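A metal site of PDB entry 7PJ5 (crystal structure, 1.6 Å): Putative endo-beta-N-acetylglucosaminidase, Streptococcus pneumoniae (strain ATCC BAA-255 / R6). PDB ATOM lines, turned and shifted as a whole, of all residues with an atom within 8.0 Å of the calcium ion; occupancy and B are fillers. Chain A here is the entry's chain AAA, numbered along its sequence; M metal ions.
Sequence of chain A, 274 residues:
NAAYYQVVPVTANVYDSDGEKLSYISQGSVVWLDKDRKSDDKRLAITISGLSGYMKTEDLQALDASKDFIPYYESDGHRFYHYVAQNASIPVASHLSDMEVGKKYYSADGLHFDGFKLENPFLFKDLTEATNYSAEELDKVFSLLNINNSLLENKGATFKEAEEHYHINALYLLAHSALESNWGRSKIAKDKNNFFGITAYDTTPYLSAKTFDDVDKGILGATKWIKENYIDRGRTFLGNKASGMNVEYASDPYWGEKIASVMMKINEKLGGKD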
ATOM      1  N   TYR A  15     -10.435   7.570  12.174  1.00  0.00           N
ATOM      2  CA  TYR A  15     -10.369   8.114  13.544  1.00  0.00           C
ATOM      3  C   TYR A  15      -8.933   8.174  14.027  1.00  0.00           C
ATOM      4  O   TYR A  15      -8.080   7.432  13.539  1.00  0.00           O
ATOM      5  CB  TYR A  15     -11.156   7.212  14.475  1.00  0.00           C
ATOM      6  CG  TYR A  15     -12.607   7.042  14.108  1.00  0.00           C
ATOM      7  CD1 TYR A  15     -13.542   7.962  14.534  1.00  0.00           C
ATOM      8  CD2 TYR A  15     -13.028   5.991  13.332  1.00  0.00           C
ATOM      9  CE1 TYR A  15     -14.878   7.829  14.209  1.00  0.00           C
ATOM     10  CE2 TYR A  15     -14.366   5.815  13.036  1.00  0.00           C
ATOM     11  CZ  TYR A  15     -15.285   6.760  13.441  1.00  0.00           C
ATOM     12  OH  TYR A  15     -16.584   6.622  13.100  1.00  0.00           O
ATOM     13  N   ASP A  16      -8.702   9.003  15.006  1.00  0.00           N
ATOM     14  CA  ASP A  16      -7.435   8.995  15.742  1.00  0.00           C
ATOM     15  C   ASP A  16      -7.523   8.037  16.939  1.00  0.00           C
ATOM     16  O   ASP A  16      -8.526   7.373  17.125  1.00  0.00           O
ATOM     17  CB  ASP A  16      -7.026  10.425  16.132  1.00  0.00           C
ATOM     18  CG  ASP A  16      -7.781  11.059  17.282  1.00  0.00           C
ATOM     19  OD1 ASP A  16      -8.648  10.365  17.887  1.00  0.00           O
ATOM     20  OD2 ASP A  16      -7.479  12.222  17.571  1.00  0.00           O
ATOM     21  N   SER A  17      -6.474   7.963  17.740  1.00  0.00           N
ATOM     22  CA  SER A  17      -6.403   6.961  18.824  1.00  0.00           C
ATOM     23  C   SER A  17      -7.406   7.282  19.936  1.00  0.00           C
ATOM     24  O   SER A  17      -7.634   6.396  20.783  1.00  0.00           O
ATOM     25  CB  SER A  17      -5.019   6.837  19.359  1.00  0.00           C
ATOM     26  OG  SER A  17      -4.582   8.100  19.784  1.00  0.00           O
ATOM     27  N   ASP A  18      -7.861   8.537  20.006  1.00  0.00           N
ATOM     28  CA  ASP A  18      -8.859   9.046  20.983  1.00  0.00           C
ATOM     29  C   ASP A  18     -10.271   8.682  20.505  1.00  0.00           C
ATOM     30  O   ASP A  18     -11.211   8.912  21.266  1.00  0.00           O
ATOM     31  CB  ASP A  18      -8.807  10.574  21.149  1.00  0.00           C
ATOM     32  CG  ASP A  18      -7.487  11.204  21.611  1.00  0.00           C
ATOM     33  OD1 ASP A  18      -6.808  10.572  22.436  1.00  0.00           O
ATOM     34  OD2 ASP A  18      -7.168  12.379  21.163  1.00  0.00           O
ATOM     35  N   GLY A  19     -10.412   8.155  19.284  1.00  0.00           N
ATOM     36  CA  GLY A  19     -11.728   7.933  18.653  1.00  0.00           C
ATOM     37  C   GLY A  19     -12.342   9.193  18.039  1.00  0.00           C
ATOM     38  O   GLY A  19     -13.535   9.185  17.701  1.00  0.00           O
ATOM     39  N   GLU A  20     -11.565  10.259  17.871  1.00  0.00           N
ATOM     40  CA  GLU A  20     -12.048  11.488  17.188  1.00  0.00           C
ATOM     41  C   GLU A  20     -11.958  11.260  15.677  1.00  0.00           C
ATOM     42  O   GLU A  20     -10.933  10.742  15.187  1.00  0.00           O
ATOM     43  CB  GLU A  20     -11.275  12.718  17.619  1.00  0.00           C
ATOM     44  CG  GLU A  20     -11.473  13.037  19.092  1.00  0.00           C
ATOM     45  CD  GLU A  20     -10.788  14.314  19.578  1.00  0.00           C
ATOM     46  OE1 GLU A  20      -9.623  14.516  19.287  1.00  0.00           O
ATOM     47  OE2 GLU A  20     -11.477  15.109  20.221  1.00  0.00           O
ATOM     48  N   LYS A  21     -12.960  11.717  14.946  1.00  0.00           N
ATOM     49  CA  LYS A  21     -12.990  11.624  13.472  1.00  0.00           C
ATOM     50  C   LYS A  21     -11.933  12.568  12.881  1.00  0.00           C
ATOM     51  O   LYS A  21     -11.955  13.760  13.182  1.00  0.00           O
ATOM     52  CB  LYS A  21     -14.387  11.975  12.990  1.00  0.00           C
ATOM     53  CG  LYS A  21     -14.535  11.883  11.492  1.00  0.00           C
ATOM     54  CD  LYS A  21     -15.969  11.878  11.082  1.00  0.00           C
ATOM     55  CE  LYS A  21     -16.172  12.174   9.615  1.00  0.00           C
ATOM     56  NZ  LYS A  21     -17.604  12.311   9.287  1.00  0.00           N
ATOM     57  N   LEU A  22     -11.101  12.042  11.991  1.00  0.00           N
ATOM     58  CA  LEU A  22     -10.071  12.799  11.246  1.00  0.00           C
ATOM     59  C   LEU A  22     -10.552  13.085   9.834  1.00  0.00           C
ATOM     60  O   LEU A  22     -10.331  14.211   9.336  1.00  0.00           O
ATOM     61  CB  LEU A  22      -8.815  11.952  11.187  1.00  0.00           C
ATOM     62  CG  LEU A  22      -8.172  11.729  12.527  1.00  0.00           C
ATOM     63  CD1 LEU A  22      -6.916  10.877  12.417  1.00  0.00           C
ATOM     64  CD2 LEU A  22      -7.946  13.053  13.248  1.00  0.00           C
HETATM   65 CA    CA M   1      -7.387  13.964  19.068  1.00  0.00          CA
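The side-chain carboxylate (OD1) of Asp 16 sits at hydrogen-bond distance from the backbone NH (N) of Gly 19, 3.2 Å away.
Three residues have an atom within 4 Å of the calcium ion: Asp 16, Asp 18 and Glu 20. The nearest printed residue that does not touch the calcium ion is Leu 22 (5.9 Å).
The calcium ion is bound by OD2 of Asp 16 (2.3 Å), OE1 of Glu 20 (2.3 Å) and OD2 of Asp 18 (2.6 Å).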
